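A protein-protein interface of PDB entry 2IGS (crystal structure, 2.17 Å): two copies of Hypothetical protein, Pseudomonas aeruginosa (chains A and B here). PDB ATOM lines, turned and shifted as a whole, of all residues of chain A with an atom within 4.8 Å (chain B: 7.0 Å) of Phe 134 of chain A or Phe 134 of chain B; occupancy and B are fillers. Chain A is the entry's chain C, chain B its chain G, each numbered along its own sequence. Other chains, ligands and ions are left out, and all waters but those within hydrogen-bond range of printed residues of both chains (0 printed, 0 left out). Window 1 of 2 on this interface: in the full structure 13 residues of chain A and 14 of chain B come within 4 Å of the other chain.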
ATOM      1  N   PRO A 125      24.723  23.575 -17.322  1.00  0.00           N
ATOM      2  CA  PRO A 125      25.918  23.039 -16.671  1.00  0.00           C
ATOM      3  C   PRO A 125      27.246  23.557 -17.314  1.00  0.00           C
ATOM      4  O   PRO A 125      28.338  23.259 -16.826  1.00  0.00           O
ATOM      5  CB  PRO A 125      25.754  21.526 -16.869  1.00  0.00           C
ATOM      6  CG  PRO A 125      24.997  21.403 -18.169  1.00  0.00           C
ATOM      7  CD  PRO A 125      24.035  22.569 -18.161  1.00  0.00           C
ATOM      8  N   VAL A 132      30.525  20.815 -24.074  1.00  0.00           N
ATOM      9  CA  VAL A 132      29.528  19.856 -24.520  1.00  0.00           C
ATOM     10  C   VAL A 132      29.226  18.977 -23.317  1.00  0.00           C
ATOM     11  O   VAL A 132      30.105  18.267 -22.824  1.00  0.00           O
ATOM     12  CB  VAL A 132      29.997  19.034 -25.753  1.00  0.00           C
ATOM     13  CG1 VAL A 132      28.896  18.083 -26.201  1.00  0.00           C
ATOM     14  CG2 VAL A 132      30.368  19.958 -26.911  1.00  0.00           C
ATOM     15  N   GLY A 133      28.001  19.070 -22.801  1.00  0.00           N
ATOM     16  CA  GLY A 133      27.637  18.245 -21.654  1.00  0.00           C
ATOM     17  C   GLY A 133      26.410  17.400 -21.923  1.00  0.00           C
ATOM     18  O   GLY A 133      26.108  17.060 -23.083  1.00  0.00           O
ATOM     19  N   PHE A 134      25.714  17.070 -20.839  1.00  0.00           N
ATOM     20  CA  PHE A 134      24.527  16.199 -20.881  1.00  0.00           C
ATOM     21  C   PHE A 134      23.317  16.945 -20.382  1.00  0.00           C
ATOM     22  O   PHE A 134      23.360  17.648 -19.378  1.00  0.00           O
ATOM     23  CB  PHE A 134      24.748  14.911 -20.076  1.00  0.00           C
ATOM     24  CG  PHE A 134      26.066  14.266 -20.353  1.00  0.00           C
ATOM     25  CD1 PHE A 134      27.055  14.258 -19.393  1.00  0.00           C
ATOM     26  CD2 PHE A 134      26.345  13.745 -21.601  1.00  0.00           C
ATOM     27  CE1 PHE A 134      28.309  13.694 -19.646  1.00  0.00           C
ATOM     28  CE2 PHE A 134      27.608  13.187 -21.882  1.00  0.00           C
ATOM     29  CZ  PHE A 134      28.593  13.154 -20.899  1.00  0.00           C
ATOM     30  N   SER A 135      22.231  16.803 -21.124  1.00  0.00           N
ATOM     31  CA  SER A 135      20.971  17.430 -20.775  1.00  0.00           C
ATOM     32  C   SER A 135      20.363  16.669 -19.599  1.00  0.00           C
ATOM     33  O   SER A 135      20.726  15.508 -19.327  1.00  0.00           O
ATOM     34  CB  SER A 135      20.043  17.400 -21.983  1.00  0.00           C
ATOM     35  OG  SER A 135      19.455  16.126 -22.152  1.00  0.00           O
ATOM     36  N   THR A 136      19.449  17.330 -18.892  1.00  0.00           N
ATOM     37  CA  THR A 136      18.763  16.706 -17.781  1.00  0.00           C
ATOM     38  C   THR A 136      17.435  16.202 -18.312  1.00  0.00           C
ATOM     39  O   THR A 136      16.885  16.770 -19.261  1.00  0.00           O
ATOM     40  CB  THR A 136      18.570  17.690 -16.620  1.00  0.00           C
ATOM     41  OG1 THR A 136      18.057  18.916 -17.145  1.00  0.00           O
ATOM     42  CG2 THR A 136      19.929  17.969 -15.936  1.00  0.00           C
ATOM     43  N   ILE A 142      20.450  13.148 -14.869  1.00  0.00           N
ATOM     44  CA  ILE A 142      20.953  12.664 -16.161  1.00  0.00           C
ATOM     45  C   ILE A 142      20.635  11.180 -16.255  1.00  0.00           C
ATOM     46  O   ILE A 142      20.782  10.451 -15.279  1.00  0.00           O
ATOM     47  CB  ILE A 142      22.473  12.884 -16.279  1.00  0.00           C
ATOM     48  CG1 ILE A 142      22.792  14.378 -16.146  1.00  0.00           C
ATOM     49  CG2 ILE A 142      23.029  12.329 -17.623  1.00  0.00           C
ATOM     50  CD1 ILE A 142      24.255  14.658 -15.705  1.00  0.00           C
ATOM     51  N   GLY A 147      20.562  13.707 -23.453  1.00  0.00           N
ATOM     52  CA  GLY A 147      21.282  13.898 -24.689  1.00  0.00           C
ATOM     53  C   GLY A 147      22.272  15.032 -24.541  1.00  0.00           C
ATOM     54  O   GLY A 147      22.763  15.309 -23.428  1.00  0.00           O
ATOM     55  N   LEU A 149      23.919  18.589 -24.291  1.00  0.00           N
ATOM     56  CA  LEU A 149      23.694  19.969 -23.863  1.00  0.00           C
ATOM     57  C   LEU A 149      24.940  20.748 -24.259  1.00  0.00           C
ATOM     58  O   LEU A 149      26.005  20.585 -23.653  1.00  0.00           O
ATOM     59  CB  LEU A 149      23.413  20.082 -22.358  1.00  0.00           C
ATOM     60  CG  LEU A 149      22.729  21.385 -21.865  1.00  0.00           C
ATOM     61  CD1 LEU A 149      23.573  22.634 -21.993  1.00  0.00           C
ATOM     62  CD2 LEU A 149      21.398  21.606 -22.545  1.00  0.00           C
ATOM     63  N   LEU A 185      21.814   9.301 -24.709  1.00  0.00           N
ATOM     64  CA  LEU A 185      23.118   8.830 -24.204  1.00  0.00           C
ATOM     65  C   LEU A 185      23.431   7.406 -24.599  1.00  0.00           C
ATOM     66  O   LEU A 185      24.600   7.078 -24.816  1.00  0.00           O
ATOM     67  CB  LEU A 185      23.261   8.942 -22.673  1.00  0.00           C
ATOM     68  CG  LEU A 185      23.280  10.315 -21.999  1.00  0.00           C
ATOM     69  CD1 LEU A 185      23.916  10.256 -20.611  1.00  0.00           C
ATOM     70  CD2 LEU A 185      23.945  11.372 -22.849  1.00  0.00           C
ATOM     71  N   PHE A 190      26.385   7.543 -30.003  1.00  0.00           N
ATOM     72  CA  PHE A 190      26.406   8.753 -29.154  1.00  0.00           C
ATOM     73  C   PHE A 190      27.813   9.257 -28.832  1.00  0.00           C
ATOM     74  O   PHE A 190      28.092  10.445 -28.954  1.00  0.00           O
ATOM     75  CB  PHE A 190      25.597   8.621 -27.856  1.00  0.00           C
ATOM     76  CG  PHE A 190      25.646   9.867 -26.995  1.00  0.00           C
ATOM     77  CD1 PHE A 190      24.723  10.873 -27.167  1.00  0.00           C
ATOM     78  CD2 PHE A 190      26.650  10.038 -26.052  1.00  0.00           C
ATOM     79  CE1 PHE A 190      24.770  12.021 -26.402  1.00  0.00           C
ATOM     80  CE2 PHE A 190      26.713  11.177 -25.277  1.00  0.00           C
ATOM     81  CZ  PHE A 190      25.772  12.181 -25.452  1.00  0.00           C
ATOM     82  N   PHE A 194      29.104  12.876 -29.875  1.00  0.00           N
ATOM     83  CA  PHE A 194      29.654  13.683 -28.782  1.00  0.00           C
ATOM     84  C   PHE A 194      31.086  14.180 -29.060  1.00  0.00           C
ATOM     85  O   PHE A 194      31.385  15.362 -28.914  1.00  0.00           O
ATOM     86  CB  PHE A 194      29.661  12.857 -27.490  1.00  0.00           C
ATOM     87  CG  PHE A 194      29.945  13.657 -26.263  1.00  0.00           C
ATOM     88  CD1 PHE A 194      31.215  14.124 -25.993  1.00  0.00           C
ATOM     89  CD2 PHE A 194      28.942  13.948 -25.366  1.00  0.00           C
ATOM     90  CE1 PHE A 194      31.481  14.871 -24.850  1.00  0.00           C
ATOM     91  CE2 PHE A 194      29.205  14.700 -24.207  1.00  0.00           C
ATOM     92  CZ  PHE A 194      30.485  15.146 -23.961  1.00  0.00           C
ATOM     93  N   PRO B 125      28.182  -3.719 -23.658  1.00  0.00           N
ATOM     94  CA  PRO B 125      27.537  -3.056 -24.773  1.00  0.00           C
ATOM     95  C   PRO B 125      28.545  -2.459 -25.779  1.00  0.00           C
ATOM     96  O   PRO B 125      28.137  -1.954 -26.832  1.00  0.00           O
ATOM     97  CB  PRO B 125      26.689  -1.978 -24.087  1.00  0.00           C
ATOM     98  CG  PRO B 125      27.409  -1.667 -22.843  1.00  0.00           C
ATOM     99  CD  PRO B 125      28.130  -2.926 -22.420  1.00  0.00           C
ATOM    100  N   ASN B 126      29.842  -2.537 -25.471  1.00  0.00           N
ATOM    101  CA  ASN B 126      30.881  -2.044 -26.386  1.00  0.00           C
ATOM    102  C   ASN B 126      31.236  -3.079 -27.421  1.00  0.00           C
ATOM    103  O   ASN B 126      31.661  -4.146 -27.079  1.00  0.00           O
ATOM    104  CB  ASN B 126      32.127  -1.564 -25.619  1.00  0.00           C
ATOM    105  CG  ASN B 126      31.878  -0.233 -24.921  1.00  0.00           C
ATOM    106  OD1 ASN B 126      30.938   0.473 -25.275  1.00  0.00           O
ATOM    107  ND2 ASN B 126      32.697   0.104 -23.935  1.00  0.00           N
ATOM    108  N   VAL B 132      34.340   3.947 -25.923  1.00  0.00           N
ATOM    109  CA  VAL B 132      34.219   4.645 -24.674  1.00  0.00           C
ATOM    110  C   VAL B 132      32.737   4.968 -24.584  1.00  0.00           C
ATOM    111  O   VAL B 132      32.189   5.665 -25.435  1.00  0.00           O
ATOM    112  CB  VAL B 132      35.071   5.952 -24.634  1.00  0.00           C
ATOM    113  CG1 VAL B 132      34.900   6.629 -23.295  1.00  0.00           C
ATOM    114  CG2 VAL B 132      36.551   5.648 -24.827  1.00  0.00           C
ATOM    115  N   GLY B 133      32.085   4.413 -23.570  1.00  0.00           N
ATOM    116  CA  GLY B 133      30.715   4.752 -23.286  1.00  0.00           C
ATOM    117  C   GLY B 133      30.532   4.998 -21.807  1.00  0.00           C
ATOM    118  O   GLY B 133      31.493   5.344 -21.082  1.00  0.00           O
ATOM    119  N   PHE B 134      29.290   4.810 -21.363  1.00  0.00           N
ATOM    120  CA  PHE B 134      28.893   5.121 -19.991  1.00  0.00           C
ATOM    121  C   PHE B 134      28.738   3.860 -19.144  1.00  0.00           C
ATOM    122  O   PHE B 134      28.184   2.856 -19.599  1.00  0.00           O
ATOM    123  CB  PHE B 134      27.576   5.902 -19.998  1.00  0.00           C
ATOM    124  CG  PHE B 134      27.667   7.211 -20.694  1.00  0.00           C
ATOM    125  CD1 PHE B 134      27.135   7.372 -21.966  1.00  0.00           C
ATOM    126  CD2 PHE B 134      28.324   8.292 -20.088  1.00  0.00           C
ATOM    127  CE1 PHE B 134      27.235   8.599 -22.643  1.00  0.00           C
ATOM    128  CE2 PHE B 134      28.425   9.545 -20.745  1.00  0.00           C
ATOM    129  CZ  PHE B 134      27.885   9.691 -22.033  1.00  0.00           C
ATOM    130  N   SER B 135      29.259   3.888 -17.930  1.00  0.00           N
ATOM    131  CA  SER B 135      28.931   2.821 -17.016  1.00  0.00           C
ATOM    132  C   SER B 135      27.422   2.915 -16.674  1.00  0.00           C
ATOM    133  O   SER B 135      26.790   4.001 -16.807  1.00  0.00           O
ATOM    134  CB  SER B 135      29.823   2.844 -15.780  1.00  0.00           C
ATOM    135  OG  SER B 135      29.551   3.978 -14.990  1.00  0.00           O
ATOM    136  N   THR B 136      26.858   1.777 -16.264  1.00  0.00           N
ATOM    137  CA  THR B 136      25.457   1.660 -15.989  1.00  0.00           C
ATOM    138  C   THR B 136      25.252   1.413 -14.500  1.00  0.00           C
ATOM    139  O   THR B 136      26.188   0.997 -13.790  1.00  0.00           O
ATOM    140  CB  THR B 136      24.765   0.553 -16.850  1.00  0.00           C
ATOM    141  OG1 THR B 136      25.348  -0.716 -16.582  1.00  0.00           O
ATOM    142  CG2 THR B 136      24.917   0.830 -18.345  1.00  0.00           C
ATOM    143  N   GLY B 141      20.637   1.247 -16.317  1.00  0.00           N
ATOM    144  CA  GLY B 141      20.409   2.629 -16.695  1.00  0.00           C
ATOM    145  C   GLY B 141      21.666   3.457 -16.627  1.00  0.00           C
ATOM    146  O   GLY B 141      22.702   2.964 -16.236  1.00  0.00           O
ATOM    147  N   ILE B 142      21.574   4.721 -17.044  1.00  0.00           N
ATOM    148  CA  ILE B 142      22.659   5.693 -16.900  1.00  0.00           C
ATOM    149  C   ILE B 142      22.156   6.751 -15.918  1.00  0.00           C
ATOM    150  O   ILE B 142      20.997   7.105 -15.959  1.00  0.00           O
ATOM    151  CB  ILE B 142      23.021   6.303 -18.253  1.00  0.00           C
ATOM    152  CG1 ILE B 142      23.429   5.187 -19.230  1.00  0.00           C
ATOM    153  CG2 ILE B 142      24.095   7.388 -18.105  1.00  0.00           C
ATOM    154  CD1 ILE B 142      23.791   5.670 -20.646  1.00  0.00           C
ATOM    155  N   SER B 143      22.990   7.191 -14.989  1.00  0.00           N
ATOM    156  CA  SER B 143      22.636   8.294 -14.103  1.00  0.00           C
ATOM    157  C   SER B 143      23.830   9.217 -13.976  1.00  0.00           C
ATOM    158  O   SER B 143      24.843   8.980 -14.615  1.00  0.00           O
ATOM    159  CB  SER B 143      22.199   7.803 -12.719  1.00  0.00           C
ATOM    160  OG  SER B 143      23.314   7.345 -11.967  1.00  0.00           O
ATOM    161  N   SER B 146      27.053   7.556 -12.889  1.00  0.00           N
ATOM    162  CA  SER B 146      27.797   6.801 -13.918  1.00  0.00           C
ATOM    163  C   SER B 146      29.119   7.460 -14.289  1.00  0.00           C
ATOM    164  O   SER B 146      29.316   8.644 -14.040  1.00  0.00           O
ATOM    165  CB  SER B 146      26.980   6.692 -15.214  1.00  0.00           C
ATOM    166  OG  SER B 146      25.885   5.813 -15.088  1.00  0.00           O
ATOM    167  N   GLY B 147      30.010   6.694 -14.915  1.00  0.00           N
ATOM    168  CA  GLY B 147      31.231   7.257 -15.455  1.00  0.00           C
ATOM    169  C   GLY B 147      31.564   6.600 -16.773  1.00  0.00           C
ATOM    170  O   GLY B 147      30.672   6.246 -17.536  1.00  0.00           O
ATOM    171  N   LEU B 148      32.854   6.409 -17.002  1.00  0.00           N
ATOM    172  CA  LEU B 148      33.394   5.845 -18.244  1.00  0.00           C
ATOM    173  C   LEU B 148      33.484   4.315 -18.231  1.00  0.00           C
ATOM    174  O   LEU B 148      33.983   3.705 -17.288  1.00  0.00           O
ATOM    175  CB  LEU B 148      34.762   6.454 -18.539  1.00  0.00           C
ATOM    176  CG  LEU B 148      34.711   7.954 -18.844  1.00  0.00           C
ATOM    177  CD1 LEU B 148      36.039   8.647 -18.667  1.00  0.00           C
ATOM    178  CD2 LEU B 148      34.174   8.187 -20.259  1.00  0.00           C
ATOM    179  N   LEU B 149      32.937   3.713 -19.277  1.00  0.00           N
ATOM    180  CA  LEU B 149      33.069   2.290 -19.525  1.00  0.00           C
ATOM    181  C   LEU B 149      33.867   2.159 -20.822  1.00  0.00           C
ATOM    182  O   LEU B 149      33.408   2.524 -21.904  1.00  0.00           O
ATOM    183  CB  LEU B 149      31.683   1.610 -19.618  1.00  0.00           C
ATOM    184  CG  LEU B 149      31.540   0.067 -19.597  1.00  0.00           C
ATOM    185  CD1 LEU B 149      32.020  -0.601 -20.903  1.00  0.00           C
ATOM    186  CD2 LEU B 149      32.225  -0.623 -18.392  1.00  0.00           C
ATOM    187  N   VAL B 150      35.091   1.672 -20.713  1.00  0.00           N
ATOM    188  CA  VAL B 150      35.896   1.585 -21.916  1.00  0.00           C
ATOM    189  C   VAL B 150      36.214   0.183 -22.367  1.00  0.00           C
ATOM    190  O   VAL B 150      36.340  -0.732 -21.533  1.00  0.00           O
ATOM    191  CB  VAL B 150      37.089   2.610 -21.965  1.00  0.00           C
ATOM    192  CG1 VAL B 150      37.159   3.519 -20.702  1.00  0.00           C
ATOM    193  CG2 VAL B 150      38.370   1.958 -22.318  1.00  0.00           C
ATOM    194  N   ASN B 155      35.614  -0.656 -16.521  1.00  0.00           N
ATOM    195  CA  ASN B 155      34.800   0.324 -15.823  1.00  0.00           C
ATOM    196  C   ASN B 155      35.705   1.247 -14.988  1.00  0.00           C
ATOM    197  O   ASN B 155      36.107   0.915 -13.866  1.00  0.00           O
ATOM    198  CB  ASN B 155      33.743  -0.416 -14.971  1.00  0.00           C
ATOM    199  CG  ASN B 155      32.646   0.503 -14.444  1.00  0.00           C
ATOM    200  OD1 ASN B 155      32.914   1.634 -14.034  1.00  0.00           O
ATOM    201  ND2 ASN B 155      31.406   0.000 -14.427  1.00  0.00           N
ATOM    202  N   ARG B 184      32.739  10.833 -12.171  1.00  0.00           N
ATOM    203  CA  ARG B 184      31.292  10.989 -12.414  1.00  0.00           C
ATOM    204  C   ARG B 184      30.980  11.836 -13.679  1.00  0.00           C
ATOM    205  O   ARG B 184      31.663  12.833 -13.959  1.00  0.00           O
ATOM    206  CB  ARG B 184      30.580  11.620 -11.182  1.00  0.00           C
ATOM    207  CG  ARG B 184      30.743  10.912  -9.773  1.00  0.00           C
ATOM    208  CD  ARG B 184      31.696  11.658  -8.848  1.00  0.00           C
ATOM    209  NE  ARG B 184      32.844  12.263  -9.536  1.00  0.00           N
ATOM    210  CZ  ARG B 184      34.045  12.370  -8.987  1.00  0.00           C
ATOM    211  NH1 ARG B 184      34.256  11.878  -7.770  1.00  0.00           N
ATOM    212  NH2 ARG B 184      35.031  12.949  -9.651  1.00  0.00           N
ATOM    213  N   LEU B 185      29.934  11.446 -14.407  1.00  0.00           N
ATOM    214  CA  LEU B 185      29.635  12.175 -15.616  1.00  0.00           C
ATOM    215  C   LEU B 185      29.226  13.632 -15.397  1.00  0.00           C
ATOM    216  O   LEU B 185      29.229  14.385 -16.337  1.00  0.00           O
ATOM    217  CB  LEU B 185      28.734  11.376 -16.573  1.00  0.00           C
ATOM    218  CG  LEU B 185      27.319  10.953 -16.239  1.00  0.00           C
ATOM    219  CD1 LEU B 185      26.433  12.108 -16.492  1.00  0.00           C
ATOM    220  CD2 LEU B 185      26.926   9.820 -17.159  1.00  0.00           C
ATOM    221  N   ASP B 186      28.912  14.025 -14.160  1.00  0.00           N
ATOM    222  CA  ASP B 186      28.606  15.425 -13.845  1.00  0.00           C
ATOM    223  C   ASP B 186      29.831  16.188 -13.300  1.00  0.00           C
ATOM    224  O   ASP B 186      29.722  17.343 -12.881  1.00  0.00           O
ATOM    225  CB  ASP B 186      27.399  15.529 -12.874  1.00  0.00           C
ATOM    226  CG  ASP B 186      27.639  14.837 -11.515  1.00  0.00           C
ATOM    227  OD1 ASP B 186      28.783  14.405 -11.204  1.00  0.00           O
ATOM    228  OD2 ASP B 186      26.656  14.728 -10.746  1.00  0.00           O
ATOM    229  N   ALA B 187      30.987  15.527 -13.278  1.00  0.00           N
ATOM    230  CA  ALA B 187      32.238  16.179 -12.867  1.00  0.00           C
ATOM    231  C   ALA B 187      32.659  17.214 -13.922  1.00  0.00           C
ATOM    232  O   ALA B 187      32.476  16.974 -15.125  1.00  0.00           O
ATOM    233  CB  ALA B 187      33.329  15.151 -12.642  1.00  0.00           C
ATOM    234  N   PHE B 190      34.656  15.980 -16.859  1.00  0.00           N
ATOM    235  CA  PHE B 190      34.273  14.694 -17.433  1.00  0.00           C
ATOM    236  C   PHE B 190      34.300  14.677 -18.961  1.00  0.00           C
ATOM    237  O   PHE B 190      34.779  13.719 -19.558  1.00  0.00           O
ATOM    238  CB  PHE B 190      32.917  14.211 -16.942  1.00  0.00           C
ATOM    239  CG  PHE B 190      32.557  12.846 -17.456  1.00  0.00           C
ATOM    240  CD1 PHE B 190      32.984  11.706 -16.792  1.00  0.00           C
ATOM    241  CD2 PHE B 190      31.814  12.697 -18.634  1.00  0.00           C
ATOM    242  CE1 PHE B 190      32.660  10.430 -17.281  1.00  0.00           C
ATOM    243  CE2 PHE B 190      31.490  11.423 -19.114  1.00  0.00           C
ATOM    244  CZ  PHE B 190      31.910  10.289 -18.419  1.00  0.00           C
ATOM    245  N   SER B 191      33.757  15.722 -19.577  1.00  0.00           N
ATOM    246  CA  SER B 191      33.735  15.838 -21.042  1.00  0.00           C
ATOM    247  C   SER B 191      35.104  15.780 -21.660  1.00  0.00           C
ATOM    248  O   SER B 191      35.283  15.103 -22.678  1.00  0.00           O
ATOM    249  CB  SER B 191      33.106  17.156 -21.483  1.00  0.00           C
ATOM    250  OG  SER B 191      31.759  16.916 -21.754  1.00  0.00           O
ATOM    251  N   PHE B 194      36.636  12.139 -20.978  1.00  0.00           N
ATOM    252  CA  PHE B 194      35.942  11.282 -21.935  1.00  0.00           C
ATOM    253  C   PHE B 194      36.538  11.404 -23.329  1.00  0.00           C
ATOM    254  O   PHE B 194      36.887  10.409 -23.927  1.00  0.00           O
ATOM    255  CB  PHE B 194      34.450  11.639 -22.004  1.00  0.00           C
ATOM    256  CG  PHE B 194      33.602  10.667 -22.815  1.00  0.00           C
ATOM    257  CD1 PHE B 194      33.754  10.542 -24.195  1.00  0.00           C
ATOM    258  CD2 PHE B 194      32.594   9.910 -22.190  1.00  0.00           C
ATOM    259  CE1 PHE B 194      32.959   9.661 -24.942  1.00  0.00           C
ATOM    260  CE2 PHE B 194      31.780   9.018 -22.942  1.00  0.00           C
ATOM    261  CZ  PHE B 194      31.971   8.913 -24.328  1.00  0.00           C
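The backbone carbonyl oxygen (O) of Val 132 of chain A lies close to the side-chain hydroxyl (OG) of Ser 191 of chain B, at 2.4 Å. The backbone carbonyl oxygen (O) of Ile 142 of chain B lies close to the backbone carbonyl oxygen (O) of Ile 142 of chain A (3.4 Å).
The backbone carbonyl oxygen (O) of Ser 146 of chain B sits at hydrogen-bond distance from the backbone NH (N) of Leu 185 of chain B (2.9 Å). The backbone NH (N) of Ser 143 of chain B sits at hydrogen-bond distance from the side-chain hydroxyl (OG) of Ser 146 of chain B, 3.2 Å away.
CE2 of Phe 134 of chain A touches CZ of Phe 134 of chain B, 3.5 Å away. CE1 of Phe 134 of chain A touches O of Leu 185 of chain B (3.5 Å). CE1 of Phe 134 of chain A touches CD2 of Phe 190 of chain B, 3.8 Å away. Ser 143 of chain B touches Ile 142 of chain A (CA to O, 3.1 Å). Ile 142 of chain A touches Leu 185 of chain B (CD1 to CD1, 3.4 Å). Phe 134 of chain B touches Leu 185 of chain A. Leu 185 of chain A touches Ile 142 of chain B. CE1 of Phe 134 of chain B touches CE2 of Phe 190 of chain A (3.7 Å). CZ of Phe 194 of chain A touches OG of Ser 191 of chain B, 3.1 Å away.
Of the printed residues of chain B, Val 132 of chain A touches Ser 191. Phe 134 of chain A touches just these residues of chain B: Phe 134, Leu 185 and Phe 190. Of the printed residues of chain B, Leu 185 of chain A touches Phe 134 and Ile 142. Gly 141 of chain B touches none of the printed residues of chain A. Of the printed residues of chain A, Leu 185 of chain B touches Phe 134 and Ile 142.
Hydrophobic or aromatic side chains of chain B within 4 Å of the printed part of chain A: Phe 134, Ile 142, Leu 185 and Phe 190. Among the printed residues, 11 pairs touch across the chains. Among the printed residues, no Asp or Glu carboxylate lies within 4 Å of a Lys or Arg side-chain nitrogen of the other chain.
Phe 134 of chain A touches its own counterpart, Phe 134 of chain B. Phe 134 of chain A touches Phe 190 of chain B, and with the chains exchanged Phe 190 of chain A touches Phe 134 of chain B. Ile 142 of chain B touches its own counterpart, Ile 142 of chain A. Ile 142 of chain A touches Leu 185 of chain B, and with the chains exchanged Leu 185 of chain A touches Ile 142 of chain B. Positions printed for both chains: 125, 132, 133, 134, 135, 136, 142, 147, 149, 185, 190 and 194. Of the 11 pairs that touch across the chains among the printed residues, 8 have their exchanged pair printed and touching as well.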
